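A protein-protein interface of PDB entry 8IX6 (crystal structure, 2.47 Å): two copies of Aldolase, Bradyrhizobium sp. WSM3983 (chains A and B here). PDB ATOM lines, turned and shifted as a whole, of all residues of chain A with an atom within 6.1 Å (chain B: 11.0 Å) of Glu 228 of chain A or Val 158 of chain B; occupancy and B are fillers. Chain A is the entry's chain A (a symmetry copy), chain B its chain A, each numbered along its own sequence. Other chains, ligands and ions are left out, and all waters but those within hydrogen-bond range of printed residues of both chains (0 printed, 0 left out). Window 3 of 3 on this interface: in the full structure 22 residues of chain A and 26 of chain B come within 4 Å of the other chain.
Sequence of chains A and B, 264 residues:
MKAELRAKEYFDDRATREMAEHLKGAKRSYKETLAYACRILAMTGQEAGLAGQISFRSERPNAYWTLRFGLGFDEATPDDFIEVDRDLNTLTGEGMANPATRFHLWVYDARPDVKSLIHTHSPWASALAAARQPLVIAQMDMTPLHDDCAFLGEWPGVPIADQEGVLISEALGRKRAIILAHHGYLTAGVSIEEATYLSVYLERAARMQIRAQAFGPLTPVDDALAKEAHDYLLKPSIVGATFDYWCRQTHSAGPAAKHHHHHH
The backbone carbonyl oxygen (O) of His 182 of chain B lies within hydrogen-bond range of the backbone NH (N) of Met 140 of chain A (2.8 Å).
Among the printed residues, merely in contact across the chains: Met 140 of chain A with Trp 155 of chain B, Met 140 of chain A with Gly 157 of chain B, Leu 225 of chain A with Trp 155 of chain B, Leu 225 of chain A with Pro 156 of chain B, Glu 228 of chain A with Val 158 of chain B, Ala 229 of chain A with Trp 155 of chain B, Ala 229 of chain A with Val 158 of chain B and Tyr 232 of chain A with Val 158 of chain B.
Of the printed residues of chain B, Leu 225 of chain A touches Trp 155 (3.6 Å) and Pro 156 (3.7 Å). No residue of chain B comes within 4 Å of Ala 226 of chain A. No residue of chain B comes within 4 Å of Lys 227 of chain A. Glu 228 of chain A touches just one residue of chain B: Val 158. Gln 53 of chain B touches none of the printed residues of chain A. Printed residues of chain A within 4 Å of Pro 156 of chain B: Leu 225. Printed residues of chain A within 4 Å of Gly 157 of chain B: Met 140 (3.3 Å). Val 158 of chain B touches three residues of chain A. Asp 162 of chain B touches none of the printed residues of chain A. Of the printed residues of chain A, His 182 of chain B touches Met 140 (2.8 Å). The nearest residue of chain B that does not touch Glu 228 of chain A is Pro 159 of chain B (5.3 Å). The nearest printed residue of chain B that does not touch Met 140 of chain A is His 121 of chain B (4.1 Å).
Hydrophobic or aromatic side chains of chain A within 4 Å of the printed part of chain B: Met 140, Leu 225, Ala 229 and Tyr 232. Hydrophobic or aromatic side chains of chain B that line the printed part of chain A: Trp 155 and Val 158. Among the printed residues, no Asp or Glu carboxylate lies within 4 Å of a Lys or Arg side-chain nitrogen of the other chain.
No position is printed for both chains.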
ATOM      1  N   MET A 140      15.388  19.678   3.697  1.00  0.00           N
ATOM      2  CA  MET A 140      15.884  18.635   2.799  1.00  0.00           C
ATOM      3  C   MET A 140      16.817  17.664   3.515  1.00  0.00           C
ATOM      4  O   MET A 140      16.687  16.443   3.372  1.00  0.00           O
ATOM      5  CB  MET A 140      16.590  19.277   1.605  1.00  0.00           C
ATOM      6  CG  MET A 140      17.620  18.385   0.933  1.00  0.00           C
ATOM      7  SD  MET A 140      16.917  17.451  -0.441  1.00  0.00           S
ATOM      8  CE  MET A 140      16.279  18.781  -1.452  1.00  0.00           C
ATOM      9  N   ASP A 223       4.876  14.388   2.198  1.00  0.00           N
ATOM     10  CA  ASP A 223       5.460  13.068   2.410  1.00  0.00           C
ATOM     11  C   ASP A 223       5.997  12.462   1.118  1.00  0.00           C
ATOM     12  O   ASP A 223       7.012  11.759   1.146  1.00  0.00           O
ATOM     13  CB  ASP A 223       4.429  12.135   3.048  1.00  0.00           C
ATOM     14  CG  ASP A 223       4.097  12.522   4.478  1.00  0.00           C
ATOM     15  OD1 ASP A 223       5.038  12.729   5.271  1.00  0.00           O
ATOM     16  OD2 ASP A 223       2.899  12.624   4.810  1.00  0.00           O
ATOM     17  N   ALA A 224       5.338  12.718  -0.015  1.00  0.00           N
ATOM     18  CA  ALA A 224       5.775  12.116  -1.269  1.00  0.00           C
ATOM     19  C   ALA A 224       7.150  12.629  -1.678  1.00  0.00           C
ATOM     20  O   ALA A 224       8.031  11.843  -2.048  1.00  0.00           O
ATOM     21  CB  ALA A 224       4.746  12.380  -2.368  1.00  0.00           C
ATOM     22  N   LEU A 225       7.355  13.946  -1.620  1.00  0.00           N
ATOM     23  CA  LEU A 225       8.673  14.493  -1.925  1.00  0.00           C
ATOM     24  C   LEU A 225       9.685  14.106  -0.855  1.00  0.00           C
ATOM     25  O   LEU A 225      10.864  13.883  -1.160  1.00  0.00           O
ATOM     26  CB  LEU A 225       8.600  16.013  -2.061  1.00  0.00           C
ATOM     27  CG  LEU A 225       7.426  16.614  -2.831  1.00  0.00           C
ATOM     28  CD1 LEU A 225       7.091  17.989  -2.279  1.00  0.00           C
ATOM     29  CD2 LEU A 225       7.752  16.695  -4.311  1.00  0.00           C
ATOM     30  N   ALA A 226       9.246  14.029   0.403  1.00  0.00           N
ATOM     31  CA  ALA A 226      10.153  13.668   1.487  1.00  0.00           C
ATOM     32  C   ALA A 226      10.720  12.270   1.281  1.00  0.00           C
ATOM     33  O   ALA A 226      11.929  12.053   1.411  1.00  0.00           O
ATOM     34  CB  ALA A 226       9.430  13.766   2.829  1.00  0.00           C
ATOM     35  N   LYS A 227       9.855  11.306   0.954  1.00  0.00           N
ATOM     36  CA  LYS A 227      10.331   9.962   0.649  1.00  0.00           C
ATOM     37  C   LYS A 227      11.245   9.968  -0.570  1.00  0.00           C
ATOM     38  O   LYS A 227      12.235   9.229  -0.619  1.00  0.00           O
ATOM     39  CB  LYS A 227       9.145   9.022   0.428  1.00  0.00           C
ATOM     40  N   GLU A 228      10.928  10.803  -1.562  1.00  0.00           N
ATOM     41  CA  GLU A 228      11.780  10.924  -2.741  1.00  0.00           C
ATOM     42  C   GLU A 228      13.155  11.465  -2.365  1.00  0.00           C
ATOM     43  O   GLU A 228      14.185  10.930  -2.792  1.00  0.00           O
ATOM     44  CB  GLU A 228      11.104  11.822  -3.776  1.00  0.00           C
ATOM     45  CG  GLU A 228      11.686  11.732  -5.174  1.00  0.00           C
ATOM     46  CD  GLU A 228      10.863  12.495  -6.192  1.00  0.00           C
ATOM     47  OE1 GLU A 228       9.619  12.391  -6.148  1.00  0.00           O
ATOM     48  OE2 GLU A 228      11.458  13.204  -7.031  1.00  0.00           O
ATOM     49  N   ALA A 229      13.190  12.532  -1.563  1.00  0.00           N
ATOM     50  CA  ALA A 229      14.464  13.049  -1.078  1.00  0.00           C
ATOM     51  C   ALA A 229      15.125  12.077  -0.112  1.00  0.00           C
ATOM     52  O   ALA A 229      16.358  11.995  -0.061  1.00  0.00           O
ATOM     53  CB  ALA A 229      14.262  14.410  -0.413  1.00  0.00           C
ATOM     54  N   HIS A 230      14.324  11.343   0.660  1.00  0.00           N
ATOM     55  CA  HIS A 230      14.863  10.308   1.534  1.00  0.00           C
ATOM     56  C   HIS A 230      15.640   9.266   0.738  1.00  0.00           C
ATOM     57  O   HIS A 230      16.719   8.831   1.157  1.00  0.00           O
ATOM     58  CB  HIS A 230      13.718   9.660   2.317  1.00  0.00           C
ATOM     59  CG  HIS A 230      14.064   8.347   2.944  1.00  0.00           C
ATOM     60  ND1 HIS A 230      14.084   7.164   2.237  1.00  0.00           N
ATOM     61  CD2 HIS A 230      14.379   8.027   4.221  1.00  0.00           C
ATOM     62  CE1 HIS A 230      14.408   6.174   3.049  1.00  0.00           C
ATOM     63  NE2 HIS A 230      14.590   6.670   4.259  1.00  0.00           N
ATOM     64  N   ASP A 231      15.109   8.865  -0.418  1.00  0.00           N
ATOM     65  CA  ASP A 231      15.764   7.841  -1.223  1.00  0.00           C
ATOM     66  C   ASP A 231      17.003   8.378  -1.927  1.00  0.00           C
ATOM     67  O   ASP A 231      17.971   7.635  -2.126  1.00  0.00           O
ATOM     68  CB  ASP A 231      14.782   7.272  -2.248  1.00  0.00           C
ATOM     69  CG  ASP A 231      13.588   6.595  -1.600  1.00  0.00           C
ATOM     70  OD1 ASP A 231      13.664   6.269  -0.397  1.00  0.00           O
ATOM     71  OD2 ASP A 231      12.571   6.390  -2.296  1.00  0.00           O
ATOM     72  N   TYR A 232      16.994   9.656  -2.314  1.00  0.00           N
ATOM     73  CA  TYR A 232      18.148  10.222  -3.005  1.00  0.00           C
ATOM     74  C   TYR A 232      19.316  10.432  -2.052  1.00  0.00           C
ATOM     75  O   TYR A 232      20.470  10.174  -2.411  1.00  0.00           O
ATOM     76  CB  TYR A 232      17.769  11.540  -3.679  1.00  0.00           C
ATOM     77  CG  TYR A 232      18.960  12.351  -4.147  1.00  0.00           C
ATOM     78  CD1 TYR A 232      19.648  12.008  -5.305  1.00  0.00           C
ATOM     79  CD2 TYR A 232      19.397  13.459  -3.430  1.00  0.00           C
ATOM     80  CE1 TYR A 232      20.738  12.747  -5.737  1.00  0.00           C
ATOM     81  CE2 TYR A 232      20.487  14.202  -3.853  1.00  0.00           C
ATOM     82  CZ  TYR A 232      21.153  13.841  -5.007  1.00  0.00           C
ATOM     83  OH  TYR A 232      22.236  14.577  -5.434  1.00  0.00           O
ATOM     84  N   LEU A 233      19.037  10.902  -0.835  1.00  0.00           N
ATOM     85  CA  LEU A 233      20.097  11.213   0.113  1.00  0.00           C
ATOM     86  C   LEU A 233      20.704   9.972   0.751  1.00  0.00           C
ATOM     87  O   LEU A 233      21.820  10.047   1.279  1.00  0.00           O
ATOM     88  CB  LEU A 233      19.569  12.151   1.202  1.00  0.00           C
ATOM     89  CG  LEU A 233      19.557  13.638   0.840  1.00  0.00           C
ATOM     90  CD1 LEU A 233      19.092  14.479   2.018  1.00  0.00           C
ATOM     91  CD2 LEU A 233      20.933  14.083   0.367  1.00  0.00           C
ATOM     92  N   GLN B  53      27.596  24.039  -2.968  1.00  0.00           N
ATOM     93  CA  GLN B  53      27.855  24.218  -4.388  1.00  0.00           C
ATOM     94  C   GLN B  53      28.315  25.644  -4.651  1.00  0.00           C
ATOM     95  O   GLN B  53      27.778  26.597  -4.080  1.00  0.00           O
ATOM     96  CB  GLN B  53      26.607  23.923  -5.229  1.00  0.00           C
ATOM     97  CG  GLN B  53      25.933  22.598  -4.921  1.00  0.00           C
ATOM     98  CD  GLN B  53      24.597  22.460  -5.615  1.00  0.00           C
ATOM     99  OE1 GLN B  53      24.115  23.394  -6.256  1.00  0.00           O
ATOM    100  NE2 GLN B  53      23.982  21.292  -5.483  1.00  0.00           N
ATOM    101  N   ASN B  98      30.029  18.060  -9.632  1.00  0.00           N
ATOM    102  CA  ASN B  98      28.838  17.801  -8.835  1.00  0.00           C
ATOM    103  C   ASN B  98      27.612  17.969  -9.724  1.00  0.00           C
ATOM    104  O   ASN B  98      27.287  19.094 -10.123  1.00  0.00           O
ATOM    105  CB  ASN B  98      28.782  18.748  -7.634  1.00  0.00           C
ATOM    106  CG  ASN B  98      27.678  18.397  -6.655  1.00  0.00           C
ATOM    107  OD1 ASN B  98      26.878  17.492  -6.895  1.00  0.00           O
ATOM    108  ND2 ASN B  98      27.632  19.115  -5.538  1.00  0.00           N
ATOM    109  N   PRO B  99      26.909  16.881 -10.057  1.00  0.00           N
ATOM    110  CA  PRO B  99      25.801  16.998 -11.023  1.00  0.00           C
ATOM    111  C   PRO B  99      24.622  17.792 -10.498  1.00  0.00           C
ATOM    112  O   PRO B  99      23.784  18.224 -11.299  1.00  0.00           O
ATOM    113  CB  PRO B  99      25.408  15.541 -11.310  1.00  0.00           C
ATOM    114  CG  PRO B  99      26.206  14.683 -10.392  1.00  0.00           C
ATOM    115  CD  PRO B  99      27.041  15.530  -9.491  1.00  0.00           C
ATOM    116  N   ALA B 100      24.524  18.000  -9.184  1.00  0.00           N
ATOM    117  CA  ALA B 100      23.463  18.837  -8.643  1.00  0.00           C
ATOM    118  C   ALA B 100      23.687  20.317  -8.923  1.00  0.00           C
ATOM    119  O   ALA B 100      22.819  21.130  -8.590  1.00  0.00           O
ATOM    120  CB  ALA B 100      23.326  18.602  -7.140  1.00  0.00           C
ATOM    121  N   THR B 101      24.822  20.682  -9.515  1.00  0.00           N
ATOM    122  CA  THR B 101      25.093  22.049  -9.936  1.00  0.00           C
ATOM    123  C   THR B 101      24.702  22.304 -11.385  1.00  0.00           C
ATOM    124  O   THR B 101      24.978  23.390 -11.905  1.00  0.00           O
ATOM    125  CB  THR B 101      26.580  22.381  -9.753  1.00  0.00           C
ATOM    126  OG1 THR B 101      27.350  21.682 -10.738  1.00  0.00           O
ATOM    127  CG2 THR B 101      27.051  21.974  -8.368  1.00  0.00           C
ATOM    128  N   PHE B 103      21.833  22.847 -12.605  1.00  0.00           N
ATOM    129  CA  PHE B 103      20.823  23.895 -12.684  1.00  0.00           C
ATOM    130  C   PHE B 103      21.419  25.295 -12.647  1.00  0.00           C
ATOM    131  O   PHE B 103      20.695  26.261 -12.913  1.00  0.00           O
ATOM    132  CB  PHE B 103      19.806  23.728 -11.548  1.00  0.00           C
ATOM    133  CG  PHE B 103      20.256  24.308 -10.234  1.00  0.00           C
ATOM    134  CD1 PHE B 103      21.028  23.558  -9.362  1.00  0.00           C
ATOM    135  CD2 PHE B 103      19.891  25.592  -9.860  1.00  0.00           C
ATOM    136  CE1 PHE B 103      21.442  24.084  -8.151  1.00  0.00           C
ATOM    137  CE2 PHE B 103      20.304  26.123  -8.652  1.00  0.00           C
ATOM    138  CZ  PHE B 103      21.079  25.368  -7.796  1.00  0.00           C
ATOM    139  N   HIS B 119      25.324  27.969  -3.399  1.00  0.00           N
ATOM    140  CA  HIS B 119      24.156  27.340  -2.794  1.00  0.00           C
ATOM    141  C   HIS B 119      24.633  26.353  -1.744  1.00  0.00           C
ATOM    142  O   HIS B 119      25.311  25.376  -2.075  1.00  0.00           O
ATOM    143  CB  HIS B 119      23.295  26.630  -3.842  1.00  0.00           C
ATOM    144  CG  HIS B 119      22.491  25.495  -3.287  1.00  0.00           C
ATOM    145  ND1 HIS B 119      21.420  25.685  -2.440  1.00  0.00           N
ATOM    146  CD2 HIS B 119      22.608  24.156  -3.451  1.00  0.00           C
ATOM    147  CE1 HIS B 119      20.910  24.513  -2.109  1.00  0.00           C
ATOM    148  NE2 HIS B 119      21.613  23.568  -2.708  1.00  0.00           N
ATOM    149  N   HIS B 121      23.553  24.473   2.350  1.00  0.00           N
ATOM    150  CA  HIS B 121      22.548  24.218   3.373  1.00  0.00           C
ATOM    151  C   HIS B 121      23.107  24.599   4.739  1.00  0.00           C
ATOM    152  O   HIS B 121      23.152  23.766   5.650  1.00  0.00           O
ATOM    153  CB  HIS B 121      22.111  22.749   3.370  1.00  0.00           C
ATOM    154  CG  HIS B 121      21.668  22.241   2.032  1.00  0.00           C
ATOM    155  ND1 HIS B 121      21.214  20.953   1.845  1.00  0.00           N
ATOM    156  CD2 HIS B 121      21.602  22.841   0.820  1.00  0.00           C
ATOM    157  CE1 HIS B 121      20.891  20.781   0.576  1.00  0.00           C
ATOM    158  NE2 HIS B 121      21.118  21.912  -0.068  1.00  0.00           N
ATOM    159  N   GLU B 154       7.854  27.146  -2.490  1.00  0.00           N
ATOM    160  CA  GLU B 154       7.708  25.769  -2.942  1.00  0.00           C
ATOM    161  C   GLU B 154       9.025  25.017  -2.809  1.00  0.00           C
ATOM    162  O   GLU B 154      10.060  25.463  -3.312  1.00  0.00           O
ATOM    163  CB  GLU B 154       7.229  25.729  -4.394  1.00  0.00           C
ATOM    164  CG  GLU B 154       7.554  24.434  -5.122  1.00  0.00           C
ATOM    165  CD  GLU B 154       6.590  23.314  -4.783  1.00  0.00           C
ATOM    166  OE1 GLU B 154       5.664  23.536  -3.973  1.00  0.00           O
ATOM    167  OE2 GLU B 154       6.759  22.205  -5.331  1.00  0.00           O
ATOM    168  N   TRP B 155       8.986  23.874  -2.123  1.00  0.00           N
ATOM    169  CA  TRP B 155      10.124  22.972  -2.097  1.00  0.00           C
ATOM    170  C   TRP B 155       9.853  21.836  -3.072  1.00  0.00           C
ATOM    171  O   TRP B 155       8.979  20.998  -2.800  1.00  0.00           O
ATOM    172  CB  TRP B 155      10.364  22.426  -0.693  1.00  0.00           C
ATOM    173  CG  TRP B 155      11.430  21.381  -0.664  1.00  0.00           C
ATOM    174  CD1 TRP B 155      12.739  21.541  -1.006  1.00  0.00           C
ATOM    175  CD2 TRP B 155      11.276  20.006  -0.295  1.00  0.00           C
ATOM    176  NE1 TRP B 155      13.415  20.354  -0.863  1.00  0.00           N
ATOM    177  CE2 TRP B 155      12.538  19.395  -0.428  1.00  0.00           C
ATOM    178  CE3 TRP B 155      10.194  19.235   0.141  1.00  0.00           C
ATOM    179  CZ2 TRP B 155      12.750  18.049  -0.141  1.00  0.00           C
ATOM    180  CZ3 TRP B 155      10.407  17.898   0.424  1.00  0.00           C
ATOM    181  CH2 TRP B 155      11.674  17.319   0.282  1.00  0.00           C
ATOM    182  N   PRO B 156      10.556  21.763  -4.201  1.00  0.00           N
ATOM    183  CA  PRO B 156      10.212  20.793  -5.247  1.00  0.00           C
ATOM    184  C   PRO B 156      10.744  19.386  -5.021  1.00  0.00           C
ATOM    185  O   PRO B 156      10.584  18.541  -5.908  1.00  0.00           O
ATOM    186  CB  PRO B 156      10.854  21.419  -6.493  1.00  0.00           C
ATOM    187  CG  PRO B 156      12.057  22.120  -5.955  1.00  0.00           C
ATOM    188  CD  PRO B 156      11.665  22.647  -4.602  1.00  0.00           C
ATOM    189  N   GLY B 157      11.370  19.102  -3.882  1.00  0.00           N
ATOM    190  CA  GLY B 157      11.921  17.782  -3.643  1.00  0.00           C
ATOM    191  C   GLY B 157      13.272  17.586  -4.300  1.00  0.00           C
ATOM    192  O   GLY B 157      14.206  18.351  -4.044  1.00  0.00           O
ATOM    193  N   VAL B 158      13.394  16.565  -5.143  1.00  0.00           N
ATOM    194  CA  VAL B 158      14.618  16.338  -5.909  1.00  0.00           C
ATOM    195  C   VAL B 158      14.292  16.460  -7.391  1.00  0.00           C
ATOM    196  O   VAL B 158      14.192  15.441  -8.089  1.00  0.00           O
ATOM    197  CB  VAL B 158      15.240  14.968  -5.598  1.00  0.00           C
ATOM    198  CG1 VAL B 158      16.675  14.914  -6.102  1.00  0.00           C
ATOM    199  CG2 VAL B 158      15.187  14.693  -4.115  1.00  0.00           C
ATOM    200  N   PRO B 159      14.130  17.668  -7.914  1.00  0.00           N
ATOM    201  CA  PRO B 159      13.763  17.820  -9.322  1.00  0.00           C
ATOM    202  C   PRO B 159      14.978  17.701 -10.229  1.00  0.00           C
ATOM    203  O   PRO B 159      16.129  17.777  -9.797  1.00  0.00           O
ATOM    204  CB  PRO B 159      13.173  19.233  -9.389  1.00  0.00           C
ATOM    205  CG  PRO B 159      13.708  19.947  -8.183  1.00  0.00           C
ATOM    206  CD  PRO B 159      14.363  18.963  -7.257  1.00  0.00           C
ATOM    207  N   ILE B 160      14.695  17.518 -11.517  1.00  0.00           N
ATOM    208  CA  ILE B 160      15.741  17.535 -12.530  1.00  0.00           C
ATOM    209  C   ILE B 160      16.311  18.945 -12.614  1.00  0.00           C
ATOM    210  O   ILE B 160      15.722  19.896 -12.087  1.00  0.00           O
ATOM    211  CB  ILE B 160      15.212  17.065 -13.897  1.00  0.00           C
ATOM    212  N   ALA B 161      17.462  19.088 -13.276  1.00  0.00           N
ATOM    213  CA  ALA B 161      18.087  20.403 -13.390  1.00  0.00           C
ATOM    214  C   ALA B 161      17.179  21.396 -14.103  1.00  0.00           C
ATOM    215  O   ALA B 161      17.256  22.603 -13.844  1.00  0.00           O
ATOM    216  CB  ALA B 161      19.426  20.289 -14.119  1.00  0.00           C
ATOM    217  N   ASP B 162      16.310  20.911 -14.992  1.00  0.00           N
ATOM    218  CA  ASP B 162      15.394  21.795 -15.704  1.00  0.00           C
ATOM    219  C   ASP B 162      14.396  22.435 -14.746  1.00  0.00           C
ATOM    220  O   ASP B 162      14.291  23.664 -14.663  1.00  0.00           O
ATOM    221  CB  ASP B 162      14.664  21.017 -16.800  1.00  0.00           C
ATOM    222  CG  ASP B 162      15.613  20.341 -17.768  1.00  0.00           C
ATOM    223  OD1 ASP B 162      16.486  19.574 -17.311  1.00  0.00           O
ATOM    224  OD2 ASP B 162      15.483  20.574 -18.988  1.00  0.00           O
ATOM    225  N   GLN B 163      13.654  21.606 -14.007  1.00  0.00           N
ATOM    226  CA  GLN B 163      12.634  22.120 -13.098  1.00  0.00           C
ATOM    227  C   GLN B 163      13.254  22.971 -11.998  1.00  0.00           C
ATOM    228  O   GLN B 163      12.752  24.054 -11.676  1.00  0.00           O
ATOM    229  CB  GLN B 163      11.839  20.961 -12.498  1.00  0.00           C
ATOM    230  CG  GLN B 163      10.993  21.341 -11.290  1.00  0.00           C
ATOM    231  CD  GLN B 163       9.697  22.025 -11.673  1.00  0.00           C
ATOM    232  OE1 GLN B 163       9.667  23.230 -11.921  1.00  0.00           O
ATOM    233  NE2 GLN B 163       8.615  21.256 -11.726  1.00  0.00           N
ATOM    234  N   GLU B 164      14.349  22.493 -11.403  1.00  0.00           N
ATOM    235  CA  GLU B 164      14.997  23.252 -10.339  1.00  0.00           C
ATOM    236  C   GLU B 164      15.588  24.551 -10.873  1.00  0.00           C
ATOM    237  O   GLU B 164      15.504  25.594 -10.214  1.00  0.00           O
ATOM    238  CB  GLU B 164      16.077  22.398  -9.673  1.00  0.00           C
ATOM    239  CG  GLU B 164      17.224  23.191  -9.083  1.00  0.00           C
ATOM    240  CD  GLU B 164      17.968  22.423  -8.012  1.00  0.00           C
ATOM    241  OE1 GLU B 164      18.625  21.416  -8.348  1.00  0.00           O
ATOM    242  OE2 GLU B 164      17.895  22.827  -6.832  1.00  0.00           O
ATOM    243  N   GLY B 165      16.178  24.509 -12.069  1.00  0.00           N
ATOM    244  CA  GLY B 165      16.754  25.716 -12.639  1.00  0.00           C
ATOM    245  C   GLY B 165      15.708  26.754 -13.001  1.00  0.00           C
ATOM    246  O   GLY B 165      15.900  27.948 -12.760  1.00  0.00           O
ATOM    247  N   LEU B 167      12.600  26.984 -11.715  1.00  0.00           N
ATOM    248  CA  LEU B 167      11.908  27.442 -10.514  1.00  0.00           C
ATOM    249  C   LEU B 167      12.703  28.519  -9.787  1.00  0.00           C
ATOM    250  O   LEU B 167      12.139  29.529  -9.351  1.00  0.00           O
ATOM    251  CB  LEU B 167      11.638  26.259  -9.584  1.00  0.00           C
ATOM    252  CG  LEU B 167      10.275  26.204  -8.891  1.00  0.00           C
ATOM    253  CD1 LEU B 167       9.149  26.165  -9.912  1.00  0.00           C
ATOM    254  CD2 LEU B 167      10.201  25.006  -7.955  1.00  0.00           C
ATOM    255  N   ILE B 168      14.016  28.326  -9.651  1.00  0.00           N
ATOM    256  CA  ILE B 168      14.828  29.287  -8.911  1.00  0.00           C
ATOM    257  C   ILE B 168      15.024  30.564  -9.719  1.00  0.00           C
ATOM    258  O   ILE B 168      15.007  31.668  -9.165  1.00  0.00           O
ATOM    259  CB  ILE B 168      16.170  28.650  -8.506  1.00  0.00           C
ATOM    260  CG1 ILE B 168      15.921  27.406  -7.652  1.00  0.00           C
ATOM    261  CG2 ILE B 168      17.036  29.651  -7.752  1.00  0.00           C
ATOM    262  CD1 ILE B 168      17.176  26.791  -7.077  1.00  0.00           C
ATOM    263  N   ALA B 181      12.704  27.547   0.636  1.00  0.00           N
ATOM    264  CA  ALA B 181      11.994  26.945   1.757  1.00  0.00           C
ATOM    265  C   ALA B 181      12.282  25.452   1.845  1.00  0.00           C
ATOM    266  O   ALA B 181      12.373  24.759   0.828  1.00  0.00           O
ATOM    267  CB  ALA B 181      10.489  27.183   1.614  1.00  0.00           C
ATOM    268  N   HIS B 182      12.436  24.967   3.078  1.00  0.00           N
ATOM    269  CA  HIS B 182      12.743  23.568   3.374  1.00  0.00           C
ATOM    270  C   HIS B 182      14.035  23.101   2.712  1.00  0.00           C
ATOM    271  O   HIS B 182      14.210  21.904   2.465  1.00  0.00           O
ATOM    272  CB  HIS B 182      11.589  22.642   2.966  1.00  0.00           C
ATOM    273  CG  HIS B 182      10.241  23.117   3.410  1.00  0.00           C
ATOM    274  ND1 HIS B 182       9.843  23.099   4.730  1.00  0.00           N
ATOM    275  CD2 HIS B 182       9.196  23.614   2.708  1.00  0.00           C
ATOM    276  CE1 HIS B 182       8.612  23.570   4.822  1.00  0.00           C
ATOM    277  NE2 HIS B 182       8.196  23.888   3.609  1.00  0.00           N
ATOM    278  N   HIS B 183      14.956  24.018   2.421  1.00  0.00           N
ATOM    279  CA  HIS B 183      16.136  23.664   1.646  1.00  0.00           C
ATOM    280  C   HIS B 183      17.363  24.424   2.130  1.00  0.00           C
ATOM    281  O   HIS B 183      18.181  23.888   2.885  1.00  0.00           O
ATOM    282  CB  HIS B 183      15.888  23.941   0.162  1.00  0.00           C
ATOM    283  CG  HIS B 183      16.916  23.347  -0.746  1.00  0.00           C
ATOM    284  ND1 HIS B 183      16.959  23.618  -2.097  1.00  0.00           N
ATOM    285  CD2 HIS B 183      17.938  22.494  -0.502  1.00  0.00           C
ATOM    286  CE1 HIS B 183      17.964  22.958  -2.645  1.00  0.00           C
ATOM    287  NE2 HIS B 183      18.574  22.268  -1.699  1.00  0.00           N
